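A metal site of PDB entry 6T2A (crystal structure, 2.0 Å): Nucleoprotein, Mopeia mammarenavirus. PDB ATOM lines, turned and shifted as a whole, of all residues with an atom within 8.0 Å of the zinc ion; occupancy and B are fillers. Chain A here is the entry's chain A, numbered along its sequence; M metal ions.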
ATOM      1  N   GLU A  28       7.835 -19.242  27.123  1.00  0.00           N
ATOM      2  CA  GLU A  28       7.385 -18.334  28.166  1.00  0.00           C
ATOM      3  C   GLU A  28       6.300 -19.031  28.986  1.00  0.00           C
ATOM      4  O   GLU A  28       5.535 -19.831  28.451  1.00  0.00           O
ATOM      5  CB  GLU A  28       6.856 -17.045  27.567  1.00  0.00           C
ATOM      6  CG  GLU A  28       7.970 -16.134  27.092  1.00  0.00           C
ATOM      7  CD  GLU A  28       8.784 -15.663  28.265  1.00  0.00           C
ATOM      8  OE1 GLU A  28       8.168 -15.256  29.284  1.00  0.00           O
ATOM      9  OE2 GLU A  28      10.017 -15.714  28.189  1.00  0.00           O
ATOM     10  N   VAL A  35       2.794 -20.637  27.831  1.00  0.00           N
ATOM     11  CA  VAL A  35       1.903 -19.824  27.021  1.00  0.00           C
ATOM     12  C   VAL A  35       2.497 -19.440  25.686  1.00  0.00           C
ATOM     13  O   VAL A  35       1.772 -18.914  24.832  1.00  0.00           O
ATOM     14  CB  VAL A  35       1.437 -18.562  27.786  1.00  0.00           C
ATOM     15  CG1 VAL A  35       0.646 -18.971  29.016  1.00  0.00           C
ATOM     16  CG2 VAL A  35       2.643 -17.725  28.185  1.00  0.00           C
ATOM     17  N   GLU A  36       3.804 -19.623  25.492  1.00  0.00           N
ATOM     18  CA  GLU A  36       4.421 -19.303  24.223  1.00  0.00           C
ATOM     19  C   GLU A  36       5.627 -20.206  24.019  1.00  0.00           C
ATOM     20  O   GLU A  36       6.450 -20.349  24.915  1.00  0.00           O
ATOM     21  CB  GLU A  36       4.826 -17.826  24.142  1.00  0.00           C
ATOM     22  CG  GLU A  36       5.237 -17.464  22.767  1.00  0.00           C
ATOM     23  CD  GLU A  36       5.728 -16.046  22.611  1.00  0.00           C
ATOM     24  OE1 GLU A  36       6.274 -15.422  23.526  1.00  0.00           O
ATOM     25  OE2 GLU A  36       5.553 -15.558  21.501  1.00  0.00           O
ATOM     26  N   ILE A  37       5.704 -20.833  22.848  1.00  0.00           N
ATOM     27  CA  ILE A  37       6.816 -21.722  22.550  1.00  0.00           C
ATOM     28  C   ILE A  37       7.374 -21.396  21.172  1.00  0.00           C
ATOM     29  O   ILE A  37       6.616 -21.168  20.218  1.00  0.00           O
ATOM     30  CB  ILE A  37       6.402 -23.201  22.631  1.00  0.00           C
ATOM     31  CG1 ILE A  37       5.956 -23.541  24.070  1.00  0.00           C
ATOM     32  CG2 ILE A  37       7.530 -24.104  22.163  1.00  0.00           C
ATOM     33  CD1 ILE A  37       5.318 -24.885  24.233  1.00  0.00           C
ATOM     34  N   ALA A  38       8.699 -21.415  21.055  1.00  0.00           N
ATOM     35  CA  ALA A  38       9.391 -21.207  19.793  1.00  0.00           C
ATOM     36  C   ALA A  38      10.494 -22.243  19.669  1.00  0.00           C
ATOM     37  O   ALA A  38      11.260 -22.463  20.609  1.00  0.00           O
ATOM     38  CB  ALA A  38       9.972 -19.800  19.673  1.00  0.00           C
ATOM     39  N   HIS A  49       6.311 -21.609  16.017  1.00  0.00           N
ATOM     40  CA  HIS A  49       6.043 -20.582  17.017  1.00  0.00           C
ATOM     41  C   HIS A  49       4.532 -20.547  17.255  1.00  0.00           C
ATOM     42  O   HIS A  49       3.754 -20.387  16.321  1.00  0.00           O
ATOM     43  CB  HIS A  49       6.552 -19.215  16.530  1.00  0.00           C
ATOM     44  CG  HIS A  49       6.275 -18.097  17.484  1.00  0.00           C
ATOM     45  ND1 HIS A  49       5.853 -16.851  17.073  1.00  0.00           N
ATOM     46  CD2 HIS A  49       6.347 -18.046  18.832  1.00  0.00           C
ATOM     47  CE1 HIS A  49       5.684 -16.079  18.130  1.00  0.00           C
ATOM     48  NE2 HIS A  49       5.973 -16.780  19.211  1.00  0.00           N
ATOM     49  N   PHE A  50       4.106 -20.742  18.490  1.00  0.00           N
ATOM     50  CA  PHE A  50       2.679 -20.804  18.784  1.00  0.00           C
ATOM     51  C   PHE A  50       2.481 -20.422  20.234  1.00  0.00           C
ATOM     52  O   PHE A  50       3.456 -20.226  20.965  1.00  0.00           O
ATOM     53  CB  PHE A  50       2.098 -22.183  18.487  1.00  0.00           C
ATOM     54  CG  PHE A  50       2.779 -23.287  19.231  1.00  0.00           C
ATOM     55  CD1 PHE A  50       3.954 -23.859  18.737  1.00  0.00           C
ATOM     56  CD2 PHE A  50       2.231 -23.788  20.405  1.00  0.00           C
ATOM     57  CE1 PHE A  50       4.573 -24.907  19.403  1.00  0.00           C
ATOM     58  CE2 PHE A  50       2.851 -24.835  21.094  1.00  0.00           C
ATOM     59  CZ  PHE A  50       4.010 -25.393  20.591  1.00  0.00           C
ATOM     60  N   TYR A  51       1.209 -20.349  20.666  1.00  0.00           N
ATOM     61  CA  TYR A  51       0.810 -19.878  21.986  1.00  0.00           C
ATOM     62  C   TYR A  51      -0.155 -20.876  22.607  1.00  0.00           C
ATOM     63  O   TYR A  51      -0.609 -21.827  21.975  1.00  0.00           O
ATOM     64  CB  TYR A  51       0.142 -18.476  21.912  1.00  0.00           C
ATOM     65  CG  TYR A  51       0.850 -17.517  20.973  1.00  0.00           C
ATOM     66  CD1 TYR A  51       1.957 -16.765  21.406  1.00  0.00           C
ATOM     67  CD2 TYR A  51       0.449 -17.404  19.648  1.00  0.00           C
ATOM     68  CE1 TYR A  51       2.609 -15.884  20.534  1.00  0.00           C
ATOM     69  CE2 TYR A  51       1.100 -16.518  18.785  1.00  0.00           C
ATOM     70  CZ  TYR A  51       2.168 -15.769  19.238  1.00  0.00           C
ATOM     71  OH  TYR A  51       2.798 -14.926  18.349  1.00  0.00           O
ATOM     72  N   HIS A  68       6.527 -11.464  30.041  1.00  0.00           N
ATOM     73  CA  HIS A  68       6.169 -11.474  28.635  1.00  0.00           C
ATOM     74  C   HIS A  68       5.147 -10.424  28.245  1.00  0.00           C
ATOM     75  O   HIS A  68       4.927 -10.225  27.039  1.00  0.00           O
ATOM     76  CB  HIS A  68       5.672 -12.880  28.214  1.00  0.00           C
ATOM     77  CG  HIS A  68       4.578 -13.431  29.072  1.00  0.00           C
ATOM     78  ND1 HIS A  68       3.318 -12.861  29.145  1.00  0.00           N
ATOM     79  CD2 HIS A  68       4.533 -14.544  29.845  1.00  0.00           C
ATOM     80  CE1 HIS A  68       2.555 -13.593  29.944  1.00  0.00           C
ATOM     81  NE2 HIS A  68       3.267 -14.609  30.390  1.00  0.00           N
ATOM     82  N   ILE A  70       2.000 -10.463  27.968  1.00  0.00           N
ATOM     83  CA  ILE A  70       0.912 -10.935  27.118  1.00  0.00           C
ATOM     84  C   ILE A  70      -0.422 -10.638  27.791  1.00  0.00           C
ATOM     85  O   ILE A  70      -0.564 -10.776  29.001  1.00  0.00           O
ATOM     86  CB  ILE A  70       1.050 -12.447  26.841  1.00  0.00           C
ATOM     87  CG1 ILE A  70       2.400 -12.758  26.176  1.00  0.00           C
ATOM     88  CG2 ILE A  70      -0.109 -12.926  25.999  1.00  0.00           C
ATOM     89  CD1 ILE A  70       2.730 -14.218  26.237  1.00  0.00           C
ATOM     90  N   TRP A 136      14.714  -6.715  18.596  1.00  0.00           N
ATOM     91  CA  TRP A 136      13.345  -6.196  18.707  1.00  0.00           C
ATOM     92  C   TRP A 136      13.032  -5.170  17.609  1.00  0.00           C
ATOM     93  O   TRP A 136      11.925  -5.167  17.070  1.00  0.00           O
ATOM     94  CB  TRP A 136      13.130  -5.591  20.101  1.00  0.00           C
ATOM     95  CG  TRP A 136      12.592  -6.625  21.082  1.00  0.00           C
ATOM     96  CD1 TRP A 136      13.330  -7.530  21.834  1.00  0.00           C
ATOM     97  CD2 TRP A 136      11.216  -6.896  21.372  1.00  0.00           C
ATOM     98  NE1 TRP A 136      12.480  -8.330  22.580  1.00  0.00           N
ATOM     99  CE2 TRP A 136      11.178  -7.964  22.314  1.00  0.00           C
ATOM    100  CE3 TRP A 136      10.009  -6.358  20.928  1.00  0.00           C
ATOM    101  CZ2 TRP A 136       9.980  -8.481  22.810  1.00  0.00           C
ATOM    102  CZ3 TRP A 136       8.829  -6.864  21.431  1.00  0.00           C
ATOM    103  CH2 TRP A 136       8.827  -7.917  22.358  1.00  0.00           C
ATOM    104  N   LYS A 140      10.383  -7.401  15.789  1.00  0.00           N
ATOM    105  CA  LYS A 140       9.174  -7.393  16.617  1.00  0.00           C
ATOM    106  C   LYS A 140       7.894  -7.497  15.780  1.00  0.00           C
ATOM    107  O   LYS A 140       6.842  -7.863  16.314  1.00  0.00           O
ATOM    108  CB  LYS A 140       9.132  -6.159  17.512  1.00  0.00           C
ATOM    109  CG  LYS A 140       8.661  -4.910  16.826  1.00  0.00           C
ATOM    110  CD  LYS A 140       8.941  -3.679  17.674  1.00  0.00           C
ATOM    111  CE  LYS A 140       8.461  -2.399  16.983  1.00  0.00           C
ATOM    112  NZ  LYS A 140       8.913  -2.328  15.544  1.00  0.00           N
ATOM    113  N   LEU A 142       7.266  -9.830  13.902  1.00  0.00           N
ATOM    114  CA  LEU A 142       6.949 -11.248  13.816  1.00  0.00           C
ATOM    115  C   LEU A 142       6.073 -11.739  14.967  1.00  0.00           C
ATOM    116  O   LEU A 142       5.562 -12.855  14.881  1.00  0.00           O
ATOM    117  CB  LEU A 142       8.247 -12.077  13.786  1.00  0.00           C
ATOM    118  CG  LEU A 142       9.227 -11.869  12.617  1.00  0.00           C
ATOM    119  CD1 LEU A 142      10.511 -12.697  12.730  1.00  0.00           C
ATOM    120  CD2 LEU A 142       8.534 -12.140  11.322  1.00  0.00           C
ATOM    121  N   CYS A 143       5.921 -10.980  16.055  1.00  0.00           N
ATOM    122  CA  CYS A 143       5.031 -11.400  17.147  1.00  0.00           C
ATOM    123  C   CYS A 143       4.247 -10.232  17.705  1.00  0.00           C
ATOM    124  O   CYS A 143       4.828  -9.300  18.269  1.00  0.00           O
ATOM    125  CB  CYS A 143       5.801 -12.095  18.278  1.00  0.00           C
ATOM    126  SG  CYS A 143       4.719 -12.711  19.585  1.00  0.00           S
ATOM    127  N   ARG A 144       2.917 -10.303  17.631  1.00  0.00           N
ATOM    128  CA  ARG A 144       2.042  -9.209  18.039  1.00  0.00           C
ATOM    129  C   ARG A 144       1.527  -9.345  19.483  1.00  0.00           C
ATOM    130  O   ARG A 144       0.689  -8.548  19.907  1.00  0.00           O
ATOM    131  CB  ARG A 144       0.860  -9.102  17.072  1.00  0.00           C
ATOM    132  CG  ARG A 144       0.373 -10.445  16.586  1.00  0.00           C
ATOM    133  CD  ARG A 144      -1.083 -10.405  16.155  1.00  0.00           C
ATOM    134  NE  ARG A 144      -1.928 -10.257  17.315  1.00  0.00           N
ATOM    135  CZ  ARG A 144      -3.069 -10.920  17.497  1.00  0.00           C
ATOM    136  NH1 ARG A 144      -3.492 -11.783  16.588  1.00  0.00           N
ATOM    137  NH2 ARG A 144      -3.770 -10.706  18.604  1.00  0.00           N
ATOM    138  N   MET A 145       2.041 -10.302  20.251  1.00  0.00           N
ATOM    139  CA  MET A 145       1.333 -10.715  21.468  1.00  0.00           C
ATOM    140  C   MET A 145       1.844 -10.049  22.730  1.00  0.00           C
ATOM    141  O   MET A 145       1.237 -10.232  23.785  1.00  0.00           O
ATOM    142  CB  MET A 145       1.397 -12.244  21.629  1.00  0.00           C
ATOM    143  CG  MET A 145       0.765 -12.983  20.437  1.00  0.00           C
ATOM    144  SD  MET A 145      -1.051 -12.908  20.673  1.00  0.00           S
ATOM    145  CE  MET A 145      -1.061 -13.137  22.433  1.00  0.00           C
ATOM    146  N   HIS A 146       2.931  -9.286  22.661  1.00  0.00           N
ATOM    147  CA  HIS A 146       3.530  -8.715  23.866  1.00  0.00           C
ATOM    148  C   HIS A 146       3.125  -7.254  23.966  1.00  0.00           C
ATOM    149  O   HIS A 146       3.880  -6.341  23.625  1.00  0.00           O
ATOM    150  CB  HIS A 146       5.047  -8.915  23.800  1.00  0.00           C
ATOM    151  CG  HIS A 146       5.449 -10.331  23.521  1.00  0.00           C
ATOM    152  ND1 HIS A 146       5.554 -11.273  24.525  1.00  0.00           N
ATOM    153  CD2 HIS A 146       5.722 -10.980  22.366  1.00  0.00           C
ATOM    154  CE1 HIS A 146       5.900 -12.436  24.003  1.00  0.00           C
ATOM    155  NE2 HIS A 146       6.021 -12.280  22.704  1.00  0.00           N
ATOM    156  N   PRO A 164       9.775  -6.778  26.998  1.00  0.00           N
ATOM    157  CA  PRO A 164       9.184  -8.071  27.340  1.00  0.00           C
ATOM    158  C   PRO A 164       9.922  -9.216  26.654  1.00  0.00           C
ATOM    159  O   PRO A 164      10.533  -9.046  25.594  1.00  0.00           O
ATOM    160  CB  PRO A 164       7.736  -7.963  26.853  1.00  0.00           C
ATOM    161  CG  PRO A 164       7.739  -6.854  25.854  1.00  0.00           C
ATOM    162  CD  PRO A 164       8.899  -5.951  26.160  1.00  0.00           C
ATOM    163  N   HIS A 165       9.874 -10.381  27.285  1.00  0.00           N
ATOM    164  CA  HIS A 165      10.481 -11.587  26.740  1.00  0.00           C
ATOM    165  C   HIS A 165       9.496 -12.285  25.799  1.00  0.00           C
ATOM    166  O   HIS A 165       8.370 -12.636  26.208  1.00  0.00           O
ATOM    167  CB  HIS A 165      10.891 -12.509  27.886  1.00  0.00           C
ATOM    168  CG  HIS A 165      11.958 -11.923  28.766  1.00  0.00           C
ATOM    169  ND1 HIS A 165      12.288 -12.453  29.989  1.00  0.00           N
ATOM    170  CD2 HIS A 165      12.745 -10.837  28.600  1.00  0.00           C
ATOM    171  CE1 HIS A 165      13.252 -11.725  30.533  1.00  0.00           C
ATOM    172  NE2 HIS A 165      13.540 -10.736  29.709  1.00  0.00           N
ATOM    173  N   CYS A 166       9.908 -12.468  24.549  1.00  0.00           N
ATOM    174  CA  CYS A 166       9.182 -13.239  23.556  1.00  0.00           C
ATOM    175  C   CYS A 166       9.960 -14.516  23.264  1.00  0.00           C
ATOM    176  O   CYS A 166      11.161 -14.460  23.009  1.00  0.00           O
ATOM    177  CB  CYS A 166       8.965 -12.432  22.273  1.00  0.00           C
ATOM    178  SG  CYS A 166       8.493 -13.353  20.749  1.00  0.00           S
ATOM    179  N   ALA A 167       9.290 -15.665  23.326  1.00  0.00           N
ATOM    180  CA  ALA A 167       9.992 -16.917  23.105  1.00  0.00           C
ATOM    181  C   ALA A 167      10.715 -16.901  21.750  1.00  0.00           C
ATOM    182  O   ALA A 167      11.876 -17.351  21.653  1.00  0.00           O
ATOM    183  CB  ALA A 167       9.021 -18.104  23.192  1.00  0.00           C
ATOM    184  N   LEU A 168      10.079 -16.358  20.717  1.00  0.00           N
ATOM    185  CA  LEU A 168      10.685 -16.363  19.396  1.00  0.00           C
ATOM    186  C   LEU A 168      11.867 -15.394  19.324  1.00  0.00           C
ATOM    187  O   LEU A 168      12.979 -15.770  18.928  1.00  0.00           O
ATOM    188  CB  LEU A 168       9.648 -16.022  18.338  1.00  0.00           C
ATOM    189  CG  LEU A 168      10.284 -15.789  16.958  1.00  0.00           C
ATOM    190  CD1 LEU A 168      11.021 -17.069  16.462  1.00  0.00           C
ATOM    191  CD2 LEU A 168       9.264 -15.285  15.954  1.00  0.00           C
ATOM    192  N   LEU A 169      11.641 -14.131  19.718  1.00  0.00           N
ATOM    193  CA  LEU A 169      12.719 -13.155  19.678  1.00  0.00           C
ATOM    194  C   LEU A 169      13.850 -13.514  20.642  1.00  0.00           C
ATOM    195  O   LEU A 169      15.010 -13.177  20.389  1.00  0.00           O
ATOM    196  CB  LEU A 169      12.168 -11.764  19.979  1.00  0.00           C
ATOM    197  CG  LEU A 169      11.856 -10.907  18.740  1.00  0.00           C
ATOM    198  CD1 LEU A 169      10.959 -11.635  17.732  1.00  0.00           C
ATOM    199  CD2 LEU A 169      11.241  -9.601  19.122  1.00  0.00           C
ATOM    200  N   ASP A 170      13.544 -14.214  21.736  1.00  0.00           N
ATOM    201  CA  ASP A 170      14.618 -14.759  22.563  1.00  0.00           C
ATOM    202  C   ASP A 170      15.508 -15.700  21.744  1.00  0.00           C
ATOM    203  O   ASP A 170      16.741 -15.564  21.732  1.00  0.00           O
ATOM    204  CB  ASP A 170      14.035 -15.489  23.769  1.00  0.00           C
ATOM    205  CG  ASP A 170      13.743 -14.529  24.924  1.00  0.00           C
ATOM    206  OD1 ASP A 170      13.775 -13.303  24.687  1.00  0.00           O
ATOM    207  OD2 ASP A 170      13.485 -14.996  26.051  1.00  0.00           O
HETATM  208 ZN    ZN M   1       6.215 -13.498  21.254  1.00  0.00          ZN
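The side-chain carboxylate of Glu 36 sits at hydrogen-bond distance from the backbone NH of Ala 167 (3.0 Å).
N of Glu 28 lies within hydrogen-bond range of O of Glu 36 (2.8 Å).
The backbone NH (N) of Leu 168 lies close to the side-chain sulfur (SG) of Cys 166 (3.4 Å).
OE2 of Glu 36 lies close to NE2 of His 49 (2.6 Å).
OH of Tyr 51 lies close to SG of Cys 143 (3.2 Å).
SG of Cys 143 lies close to N of Met 145, at 3.7 Å.
A ring nitrogen (ND1) of His 146 sits at hydrogen-bond distance from the backbone carbonyl oxygen of His 68.
SG of Cys 166 sits close to N of Leu 169 (3.4 Å).
His 49 touches the zinc ion (NE2 to ZN, 3.9 Å).
Within 4 Å of the zinc ion: Glu 36, His 49, Cys 143, His 146 and Cys 166.
NE2 of His 146 is bound to the zinc ion (1.9 Å).
OE2 of Glu 36 is bound to the zinc ion.
The side-chain sulfur (SG) of Cys 166 is bound to the zinc ion (2.3 Å).
The zinc ion is bound by the side-chain sulfur (SG) of Cys 143, 2.4 Å away.
The zinc ion has four donor atoms within binding distance.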
